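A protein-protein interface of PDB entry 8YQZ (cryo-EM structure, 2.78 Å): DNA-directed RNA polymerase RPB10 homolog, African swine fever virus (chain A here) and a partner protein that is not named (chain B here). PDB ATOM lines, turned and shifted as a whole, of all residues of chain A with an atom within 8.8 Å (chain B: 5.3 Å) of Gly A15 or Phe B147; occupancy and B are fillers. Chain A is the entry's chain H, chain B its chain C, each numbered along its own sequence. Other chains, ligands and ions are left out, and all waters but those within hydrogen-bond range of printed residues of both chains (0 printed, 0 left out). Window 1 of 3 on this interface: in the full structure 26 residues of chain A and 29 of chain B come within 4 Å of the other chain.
The side-chain hydroxyl (OG) of Ser B127 is in hydrogen-bond range of the backbone carbonyl oxygen (O) of Asn B144, 2.8 Å away. N of Thr B146 is in hydrogen-bond range of OG of Ser B127 (3.5 Å). The backbone carbonyl oxygen of Phe B147 is in hydrogen-bond range of the backbone NH of Ser B127. The backbone NH (N) of Gly A15 sits at hydrogen-bond distance from the backbone carbonyl oxygen (O) of Val A5 (2.9 Å).
Among the printed residues, pairs that only touch across the chains: Leu A2 with Glu B148 (3.9 Å), Val A5 with Ile B100 (3.99 Å), Val A5 with Phe B147 (3.6 Å), Pro A13 with Pro B101 (3.9 Å), Gly A15 with Phe B147 (3.8 Å), Thr A16 with Asn B144 (3.9 Å), Thr A16 with Phe B147 (3.7 Å) and Ala A19 with Glu B148 (3.8 Å).
The backbone carbonyl oxygen (O) of Thr A16 is in hydrogen-bond range of the side-chain hydroxyl (OG1) of Thr B146 (2.9 Å).
Of the 21 printed residues of chain A, 6 touch a printed residue of chain B. Hydrophobic or aromatic side chains of chain A that line the printed part of chain B: Leu A2, Val A5, Pro A13 and Ala A19. Along chain B the printed residues that touch a printed residue of chain A span positions 100 to 148. Among the printed residues, no Asp or Glu carboxylate lies within 4 Å of a Lys or Arg side-chain nitrogen of the other chain.
Of chain B, only Phe B147 (3.8 Å) comes within 4 Å of Gly A15. Printed residues of chain B within 4 Å of Thr A16: Asn B144, Thr B146 and Phe B147. Tyr A17 touches none of the printed residues of chain B. Printed residues of chain A within 4 Å of Ile B100: Val A5. Tyr B126 touches none of the printed residues of chain A. Printed residues of chain A within 4 Å of Asn B144: Thr A16 (3.9 Å). The nearest residue of chain B that does not touch Gly A15 is Thr B146 (4.2 Å).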
ATOM      1  N   LEU A   2       6.488  -6.352  -0.350  1.00  0.00           N
ATOM      2  CA  LEU A   2       5.559  -7.421  -0.671  1.00  0.00           C
ATOM      3  C   LEU A   2       6.252  -8.738  -0.380  1.00  0.00           C
ATOM      4  O   LEU A   2       7.425  -8.773  -0.022  1.00  0.00           O
ATOM      5  CB  LEU A   2       5.118  -7.366  -2.138  1.00  0.00           C
ATOM      6  CG  LEU A   2       4.331  -6.165  -2.649  1.00  0.00           C
ATOM      7  CD1 LEU A   2       4.468  -6.051  -4.142  1.00  0.00           C
ATOM      8  CD2 LEU A   2       2.888  -6.278  -2.264  1.00  0.00           C
ATOM      9  N   ILE A   3       5.521  -9.830  -0.523  1.00  0.00           N
ATOM     10  CA  ILE A   3       6.175 -11.140  -0.495  1.00  0.00           C
ATOM     11  C   ILE A   3       7.044 -11.272  -1.738  1.00  0.00           C
ATOM     12  O   ILE A   3       6.585 -10.939  -2.840  1.00  0.00           O
ATOM     13  CB  ILE A   3       5.131 -12.259  -0.414  1.00  0.00           C
ATOM     14  CG1 ILE A   3       4.417 -12.223   0.934  1.00  0.00           C
ATOM     15  CG2 ILE A   3       5.761 -13.618  -0.596  1.00  0.00           C
ATOM     16  CD1 ILE A   3       3.250 -13.164   1.030  1.00  0.00           C
ATOM     17  N   PRO A   4       8.292 -11.719  -1.622  1.00  0.00           N
ATOM     18  CA  PRO A   4       9.180 -11.728  -2.784  1.00  0.00           C
ATOM     19  C   PRO A   4       8.665 -12.633  -3.891  1.00  0.00           C
ATOM     20  O   PRO A   4       7.836 -13.513  -3.676  1.00  0.00           O
ATOM     21  CB  PRO A   4      10.502 -12.238  -2.209  1.00  0.00           C
ATOM     22  CG  PRO A   4      10.122 -12.957  -0.988  1.00  0.00           C
ATOM     23  CD  PRO A   4       8.978 -12.218  -0.422  1.00  0.00           C
ATOM     24  N   VAL A   5       9.150 -12.368  -5.104  1.00  0.00           N
ATOM     25  CA  VAL A   5       8.750 -13.154  -6.264  1.00  0.00           C
ATOM     26  C   VAL A   5       9.244 -14.585  -6.136  1.00  0.00           C
ATOM     27  O   VAL A   5       8.533 -15.536  -6.468  1.00  0.00           O
ATOM     28  CB  VAL A   5       9.256 -12.490  -7.556  1.00  0.00           C
ATOM     29  CG1 VAL A   5       9.008 -13.374  -8.734  1.00  0.00           C
ATOM     30  CG2 VAL A   5       8.566 -11.180  -7.762  1.00  0.00           C
ATOM     31  N   VAL A   6      10.472 -14.758  -5.661  1.00  0.00           N
ATOM     32  CA  VAL A   6      11.071 -16.064  -5.448  1.00  0.00           C
ATOM     33  C   VAL A   6      11.616 -16.107  -4.030  1.00  0.00           C
ATOM     34  O   VAL A   6      11.799 -15.081  -3.379  1.00  0.00           O
ATOM     35  CB  VAL A   6      12.183 -16.375  -6.470  1.00  0.00           C
ATOM     36  CG1 VAL A   6      11.599 -16.587  -7.842  1.00  0.00           C
ATOM     37  CG2 VAL A   6      13.189 -15.270  -6.507  1.00  0.00           C
ATOM     38  N   CYS A   7      11.857 -17.317  -3.545  1.00  0.00           N
ATOM     39  CA  CYS A   7      12.489 -17.476  -2.247  1.00  0.00           C
ATOM     40  C   CYS A   7      13.895 -16.890  -2.280  1.00  0.00           C
ATOM     41  O   CYS A   7      14.680 -17.186  -3.179  1.00  0.00           O
ATOM     42  CB  CYS A   7      12.524 -18.950  -1.866  1.00  0.00           C
ATOM     43  SG  CYS A   7      13.461 -19.345  -0.393  1.00  0.00           S
ATOM     44  N   GLY A  11      15.367 -19.736  -4.546  1.00  0.00           N
ATOM     45  CA  GLY A  11      14.859 -19.306  -5.823  1.00  0.00           C
ATOM     46  C   GLY A  11      13.595 -19.983  -6.286  1.00  0.00           C
ATOM     47  O   GLY A  11      13.212 -19.801  -7.441  1.00  0.00           O
ATOM     48  N   PHE A  12      12.945 -20.764  -5.438  1.00  0.00           N
ATOM     49  CA  PHE A  12      11.657 -21.334  -5.787  1.00  0.00           C
ATOM     50  C   PHE A  12      10.622 -20.220  -5.921  1.00  0.00           C
ATOM     51  O   PHE A  12      10.606 -19.291  -5.112  1.00  0.00           O
ATOM     52  CB  PHE A  12      11.226 -22.346  -4.724  1.00  0.00           C
ATOM     53  CG  PHE A  12       9.945 -23.054  -5.033  1.00  0.00           C
ATOM     54  CD1 PHE A  12       9.942 -24.215  -5.774  1.00  0.00           C
ATOM     55  CD2 PHE A  12       8.741 -22.555  -4.581  1.00  0.00           C
ATOM     56  CE1 PHE A  12       8.769 -24.855  -6.058  1.00  0.00           C
ATOM     57  CE2 PHE A  12       7.567 -23.183  -4.870  1.00  0.00           C
ATOM     58  CZ  PHE A  12       7.582 -24.341  -5.605  1.00  0.00           C
ATOM     59  N   PRO A  13       9.756 -20.270  -6.921  1.00  0.00           N
ATOM     60  CA  PRO A  13       8.815 -19.165  -7.124  1.00  0.00           C
ATOM     61  C   PRO A  13       7.665 -19.152  -6.129  1.00  0.00           C
ATOM     62  O   PRO A  13       6.549 -19.538  -6.464  1.00  0.00           O
ATOM     63  CB  PRO A  13       8.317 -19.403  -8.552  1.00  0.00           C
ATOM     64  CG  PRO A  13       8.464 -20.843  -8.751  1.00  0.00           C
ATOM     65  CD  PRO A  13       9.678 -21.256  -8.009  1.00  0.00           C
ATOM     66  N   ILE A  14       7.908 -18.689  -4.907  1.00  0.00           N
ATOM     67  CA  ILE A  14       6.830 -18.632  -3.929  1.00  0.00           C
ATOM     68  C   ILE A  14       5.856 -17.506  -4.220  1.00  0.00           C
ATOM     69  O   ILE A  14       4.789 -17.453  -3.610  1.00  0.00           O
ATOM     70  CB  ILE A  14       7.374 -18.469  -2.501  1.00  0.00           C
ATOM     71  CG1 ILE A  14       8.315 -17.273  -2.424  1.00  0.00           C
ATOM     72  CG2 ILE A  14       8.079 -19.712  -2.060  1.00  0.00           C
ATOM     73  CD1 ILE A  14       8.431 -16.675  -1.080  1.00  0.00           C
ATOM     74  N   GLY A  15       6.191 -16.608  -5.143  1.00  0.00           N
ATOM     75  CA  GLY A  15       5.385 -15.422  -5.350  1.00  0.00           C
ATOM     76  C   GLY A  15       4.210 -15.628  -6.276  1.00  0.00           C
ATOM     77  O   GLY A  15       3.371 -14.737  -6.416  1.00  0.00           O
ATOM     78  N   THR A  16       4.132 -16.783  -6.931  1.00  0.00           N
ATOM     79  CA  THR A  16       2.960 -17.075  -7.741  1.00  0.00           C
ATOM     80  C   THR A  16       1.772 -17.491  -6.890  1.00  0.00           C
ATOM     81  O   THR A  16       0.644 -17.516  -7.389  1.00  0.00           O
ATOM     82  CB  THR A  16       3.283 -18.149  -8.785  1.00  0.00           C
ATOM     83  OG1 THR A  16       2.072 -18.705  -9.299  1.00  0.00           O
ATOM     84  CG2 THR A  16       4.105 -19.238  -8.204  1.00  0.00           C
ATOM     85  N   TYR A  17       1.992 -17.796  -5.615  1.00  0.00           N
ATOM     86  CA  TYR A  17       0.918 -18.121  -4.694  1.00  0.00           C
ATOM     87  C   TYR A  17       0.747 -17.107  -3.580  1.00  0.00           C
ATOM     88  O   TYR A  17      -0.013 -17.368  -2.651  1.00  0.00           O
ATOM     89  CB  TYR A  17       1.150 -19.491  -4.064  1.00  0.00           C
ATOM     90  CG  TYR A  17       1.760 -20.511  -4.972  1.00  0.00           C
ATOM     91  CD1 TYR A  17       3.099 -20.831  -4.880  1.00  0.00           C
ATOM     92  CD2 TYR A  17       0.994 -21.169  -5.912  1.00  0.00           C
ATOM     93  CE1 TYR A  17       3.655 -21.766  -5.698  1.00  0.00           C
ATOM     94  CE2 TYR A  17       1.543 -22.106  -6.735  1.00  0.00           C
ATOM     95  CZ  TYR A  17       2.871 -22.403  -6.623  1.00  0.00           C
ATOM     96  OH  TYR A  17       3.425 -23.341  -7.446  1.00  0.00           O
ATOM     97  N   ALA A  18       1.428 -15.967  -3.642  1.00  0.00           N
ATOM     98  CA  ALA A  18       1.459 -15.049  -2.513  1.00  0.00           C
ATOM     99  C   ALA A  18       0.094 -14.421  -2.248  1.00  0.00           C
ATOM    100  O   ALA A  18      -0.326 -14.292  -1.094  1.00  0.00           O
ATOM    101  CB  ALA A  18       2.514 -13.975  -2.755  1.00  0.00           C
ATOM    102  N   ALA A  19      -0.611 -14.008  -3.304  1.00  0.00           N
ATOM    103  CA  ALA A  19      -1.914 -13.372  -3.130  1.00  0.00           C
ATOM    104  C   ALA A  19      -2.939 -14.348  -2.568  1.00  0.00           C
ATOM    105  O   ALA A  19      -3.686 -14.022  -1.629  1.00  0.00           O
ATOM    106  CB  ALA A  19      -2.393 -12.806  -4.462  1.00  0.00           C
ATOM    107  N   ILE A  20      -2.992 -15.554  -3.136  1.00  0.00           N
ATOM    108  CA  ILE A  20      -3.896 -16.574  -2.626  1.00  0.00           C
ATOM    109  C   ILE A  20      -3.560 -16.890  -1.180  1.00  0.00           C
ATOM    110  O   ILE A  20      -4.451 -17.023  -0.339  1.00  0.00           O
ATOM    111  CB  ILE A  20      -3.846 -17.840  -3.500  1.00  0.00           C
ATOM    112  CG1 ILE A  20      -4.242 -17.532  -4.935  1.00  0.00           C
ATOM    113  CG2 ILE A  20      -4.757 -18.906  -2.945  1.00  0.00           C
ATOM    114  CD1 ILE A  20      -3.844 -18.607  -5.898  1.00  0.00           C
ATOM    115  N   PHE A  21      -2.272 -17.009  -0.866  1.00  0.00           N
ATOM    116  CA  PHE A  21      -1.885 -17.342   0.495  1.00  0.00           C
ATOM    117  C   PHE A  21      -2.306 -16.255   1.469  1.00  0.00           C
ATOM    118  O   PHE A  21      -2.795 -16.555   2.558  1.00  0.00           O
ATOM    119  CB  PHE A  21      -0.379 -17.571   0.583  1.00  0.00           C
ATOM    120  CG  PHE A  21       0.117 -17.726   1.981  1.00  0.00           C
ATOM    121  CD1 PHE A  21      -0.175 -18.863   2.705  1.00  0.00           C
ATOM    122  CD2 PHE A  21       0.837 -16.723   2.588  1.00  0.00           C
ATOM    123  CE1 PHE A  21       0.258 -18.999   3.991  1.00  0.00           C
ATOM    124  CE2 PHE A  21       1.268 -16.860   3.872  1.00  0.00           C
ATOM    125  CZ  PHE A  21       0.983 -18.000   4.571  1.00  0.00           C
ATOM    126  N   ILE A  60       3.317 -25.686  -2.313  1.00  0.00           N
ATOM    127  CA  ILE A  60       4.672 -25.277  -1.962  1.00  0.00           C
ATOM    128  C   ILE A  60       5.324 -26.406  -1.172  1.00  0.00           C
ATOM    129  O   ILE A  60       4.673 -27.002  -0.308  1.00  0.00           O
ATOM    130  CB  ILE A  60       4.647 -23.954  -1.183  1.00  0.00           C
ATOM    131  CG1 ILE A  60       4.200 -22.830  -2.110  1.00  0.00           C
ATOM    132  CG2 ILE A  60       5.998 -23.628  -0.590  1.00  0.00           C
ATOM    133  CD1 ILE A  60       3.937 -21.550  -1.417  1.00  0.00           C
ATOM    134  N   CYS A  66      11.553 -21.559   2.107  1.00  0.00           N
ATOM    135  CA  CYS A  66      10.408 -21.061   1.358  1.00  0.00           C
ATOM    136  C   CYS A  66       9.251 -20.734   2.280  1.00  0.00           C
ATOM    137  O   CYS A  66       8.599 -19.695   2.131  1.00  0.00           O
ATOM    138  CB  CYS A  66       9.989 -22.086   0.313  1.00  0.00           C
ATOM    139  SG  CYS A  66      11.290 -22.511  -0.825  1.00  0.00           S
ATOM    140  N   HIS A  69      10.055 -17.530   4.343  1.00  0.00           N
ATOM    141  CA  HIS A  69       9.892 -16.256   3.652  1.00  0.00           C
ATOM    142  C   HIS A  69       8.444 -15.999   3.262  1.00  0.00           C
ATOM    143  O   HIS A  69       8.033 -14.842   3.161  1.00  0.00           O
ATOM    144  CB  HIS A  69      10.796 -16.186   2.424  1.00  0.00           C
ATOM    145  CG  HIS A  69      12.252 -16.283   2.743  1.00  0.00           C
ATOM    146  ND1 HIS A  69      12.832 -15.580   3.773  1.00  0.00           N
ATOM    147  CD2 HIS A  69      13.248 -16.987   2.163  1.00  0.00           C
ATOM    148  CE1 HIS A  69      14.119 -15.864   3.826  1.00  0.00           C
ATOM    149  NE2 HIS A  69      14.397 -16.712   2.858  1.00  0.00           N
ATOM    150  N   LEU A  70       7.661 -17.049   3.034  1.00  0.00           N
ATOM    151  CA  LEU A  70       6.248 -16.863   2.741  1.00  0.00           C
ATOM    152  C   LEU A  70       5.460 -16.462   3.979  1.00  0.00           C
ATOM    153  O   LEU A  70       4.441 -15.777   3.872  1.00  0.00           O
ATOM    154  CB  LEU A  70       5.681 -18.146   2.150  1.00  0.00           C
ATOM    155  CG  LEU A  70       4.227 -18.153   1.728  1.00  0.00           C
ATOM    156  CD1 LEU A  70       4.043 -17.432   0.421  1.00  0.00           C
ATOM    157  CD2 LEU A  70       3.790 -19.577   1.631  1.00  0.00           C
ATOM    158  N   ILE B 100      10.562 -13.125 -12.405  1.00  0.00           N
ATOM    159  CA  ILE B 100       9.413 -13.918 -12.820  1.00  0.00           C
ATOM    160  C   ILE B 100       9.935 -15.051 -13.693  1.00  0.00           C
ATOM    161  O   ILE B 100      10.664 -14.791 -14.658  1.00  0.00           O
ATOM    162  CB  ILE B 100       8.382 -13.064 -13.569  1.00  0.00           C
ATOM    163  CG1 ILE B 100       7.732 -12.061 -12.627  1.00  0.00           C
ATOM    164  CG2 ILE B 100       7.341 -13.933 -14.217  1.00  0.00           C
ATOM    165  CD1 ILE B 100       6.845 -11.080 -13.326  1.00  0.00           C
ATOM    166  N   PRO B 101       9.619 -16.310 -13.394  1.00  0.00           N
ATOM    167  CA  PRO B 101      10.086 -17.406 -14.247  1.00  0.00           C
ATOM    168  C   PRO B 101       9.287 -17.455 -15.538  1.00  0.00           C
ATOM    169  O   PRO B 101       8.057 -17.436 -15.524  1.00  0.00           O
ATOM    170  CB  PRO B 101       9.842 -18.652 -13.392  1.00  0.00           C
ATOM    171  CG  PRO B 101       9.506 -18.161 -12.055  1.00  0.00           C
ATOM    172  CD  PRO B 101       8.907 -16.825 -12.219  1.00  0.00           C
ATOM    173  N   ILE B 125      -1.170  -4.364  -8.944  1.00  0.00           N
ATOM    174  CA  ILE B 125      -0.822  -4.739 -10.309  1.00  0.00           C
ATOM    175  C   ILE B 125      -0.401  -6.199 -10.313  1.00  0.00           C
ATOM    176  O   ILE B 125       0.427  -6.613  -9.499  1.00  0.00           O
ATOM    177  CB  ILE B 125       0.303  -3.851 -10.858  1.00  0.00           C
ATOM    178  CG1 ILE B 125       0.027  -2.382 -10.555  1.00  0.00           C
ATOM    179  CG2 ILE B 125       0.464  -4.062 -12.337  1.00  0.00           C
ATOM    180  CD1 ILE B 125       1.232  -1.520 -10.701  1.00  0.00           C
ATOM    181  N   TYR B 126      -0.967  -6.978 -11.222  1.00  0.00           N
ATOM    182  CA  TYR B 126      -0.618  -8.378 -11.377  1.00  0.00           C
ATOM    183  C   TYR B 126       0.057  -8.590 -12.725  1.00  0.00           C
ATOM    184  O   TYR B 126      -0.002  -7.744 -13.613  1.00  0.00           O
ATOM    185  CB  TYR B 126      -1.858  -9.254 -11.224  1.00  0.00           C
ATOM    186  CG  TYR B 126      -2.469  -9.185  -9.852  1.00  0.00           C
ATOM    187  CD1 TYR B 126      -1.887  -9.833  -8.783  1.00  0.00           C
ATOM    188  CD2 TYR B 126      -3.620  -8.455  -9.623  1.00  0.00           C
ATOM    189  CE1 TYR B 126      -2.438  -9.767  -7.532  1.00  0.00           C
ATOM    190  CE2 TYR B 126      -4.175  -8.381  -8.373  1.00  0.00           C
ATOM    191  CZ  TYR B 126      -3.581  -9.039  -7.332  1.00  0.00           C
ATOM    192  OH  TYR B 126      -4.134  -8.972  -6.082  1.00  0.00           O
ATOM    193  N   SER B 127       0.721  -9.734 -12.880  1.00  0.00           N
ATOM    194  CA  SER B 127       1.425 -10.006 -14.125  1.00  0.00           C
ATOM    195  C   SER B 127       0.484 -10.218 -15.296  1.00  0.00           C
ATOM    196  O   SER B 127       0.926 -10.152 -16.443  1.00  0.00           O
ATOM    197  CB  SER B 127       2.337 -11.219 -13.980  1.00  0.00           C
ATOM    198  OG  SER B 127       1.741 -12.221 -13.197  1.00  0.00           O
ATOM    199  N   ASN B 144       3.081 -16.967 -15.558  1.00  0.00           N
ATOM    200  CA  ASN B 144       1.813 -17.066 -14.860  1.00  0.00           C
ATOM    201  C   ASN B 144       1.196 -15.688 -14.627  1.00  0.00           C
ATOM    202  O   ASN B 144       1.908 -14.689 -14.522  1.00  0.00           O
ATOM    203  CB  ASN B 144       1.999 -17.775 -13.528  1.00  0.00           C
ATOM    204  CG  ASN B 144       2.032 -19.263 -13.672  1.00  0.00           C
ATOM    205  OD1 ASN B 144       1.263 -19.836 -14.421  1.00  0.00           O
ATOM    206  ND2 ASN B 144       2.919 -19.901 -12.944  1.00  0.00           N
ATOM    207  N   PRO B 145      -0.128 -15.611 -14.531  1.00  0.00           N
ATOM    208  CA  PRO B 145      -0.780 -14.307 -14.375  1.00  0.00           C
ATOM    209  C   PRO B 145      -1.030 -13.882 -12.936  1.00  0.00           C
ATOM    210  O   PRO B 145      -1.732 -12.897 -12.699  1.00  0.00           O
ATOM    211  CB  PRO B 145      -2.100 -14.513 -15.116  1.00  0.00           C
ATOM    212  CG  PRO B 145      -2.410 -15.921 -14.889  1.00  0.00           C
ATOM    213  CD  PRO B 145      -1.106 -16.666 -14.838  1.00  0.00           C
ATOM    214  N   THR B 146      -0.467 -14.598 -11.969  1.00  0.00           N
ATOM    215  CA  THR B 146      -0.825 -14.416 -10.570  1.00  0.00           C
ATOM    216  C   THR B 146       0.211 -13.647  -9.764  1.00  0.00           C
ATOM    217  O   THR B 146       0.011 -13.446  -8.566  1.00  0.00           O
ATOM    218  CB  THR B 146      -1.087 -15.776  -9.926  1.00  0.00           C
ATOM    219  OG1 THR B 146       0.055 -16.615 -10.106  1.00  0.00           O
ATOM    220  CG2 THR B 146      -2.274 -16.441 -10.557  1.00  0.00           C
ATOM    221  N   PHE B 147       1.305 -13.209 -10.378  1.00  0.00           N
ATOM    222  CA  PHE B 147       2.366 -12.522  -9.653  1.00  0.00           C
ATOM    223  C   PHE B 147       1.943 -11.107  -9.291  1.00  0.00           C
ATOM    224  O   PHE B 147       1.289 -10.432 -10.083  1.00  0.00           O
ATOM    225  CB  PHE B 147       3.641 -12.465 -10.492  1.00  0.00           C
ATOM    226  CG  PHE B 147       4.394 -13.754 -10.555  1.00  0.00           C
ATOM    227  CD1 PHE B 147       5.336 -14.068  -9.601  1.00  0.00           C
ATOM    228  CD2 PHE B 147       4.167 -14.649 -11.575  1.00  0.00           C
ATOM    229  CE1 PHE B 147       6.025 -15.245  -9.666  1.00  0.00           C
ATOM    230  CE2 PHE B 147       4.852 -15.818 -11.638  1.00  0.00           C
ATOM    231  CZ  PHE B 147       5.779 -16.117 -10.682  1.00  0.00           C
ATOM    232  N   GLU B 148       2.335 -10.652  -8.107  1.00  0.00           N
ATOM    233  CA  GLU B 148       2.153  -9.260  -7.699  1.00  0.00           C
ATOM    234  C   GLU B 148       3.377  -8.479  -8.144  1.00  0.00           C
ATOM    235  O   GLU B 148       4.504  -8.773  -7.754  1.00  0.00           O
ATOM    236  CB  GLU B 148       1.968  -9.149  -6.194  1.00  0.00           C
ATOM    237  CG  GLU B 148       0.654  -9.647  -5.669  1.00  0.00           C
ATOM    238  CD  GLU B 148       0.622  -9.695  -4.159  1.00  0.00           C
ATOM    239  OE1 GLU B 148       1.696  -9.803  -3.539  1.00  0.00           O
ATOM    240  OE2 GLU B 148      -0.477  -9.608  -3.580  1.00  0.00           O
ATOM    241  N   ILE B 149       3.159  -7.459  -8.968  1.00  0.00           N
ATOM    242  CA  ILE B 149       4.275  -6.644  -9.424  1.00  0.00           C
ATOM    243  C   ILE B 149       4.389  -5.381  -8.584  1.00  0.00           C
ATOM    244  O   ILE B 149       5.492  -4.895  -8.318  1.00  0.00           O
ATOM    245  CB  ILE B 149       4.125  -6.336 -10.924  1.00  0.00           C
ATOM    246  CG1 ILE B 149       4.281  -7.620 -11.734  1.00  0.00           C
ATOM    247  CG2 ILE B 149       5.147  -5.313 -11.378  1.00  0.00           C
ATOM    248  CD1 ILE B 149       4.042  -7.450 -13.187  1.00  0.00           C
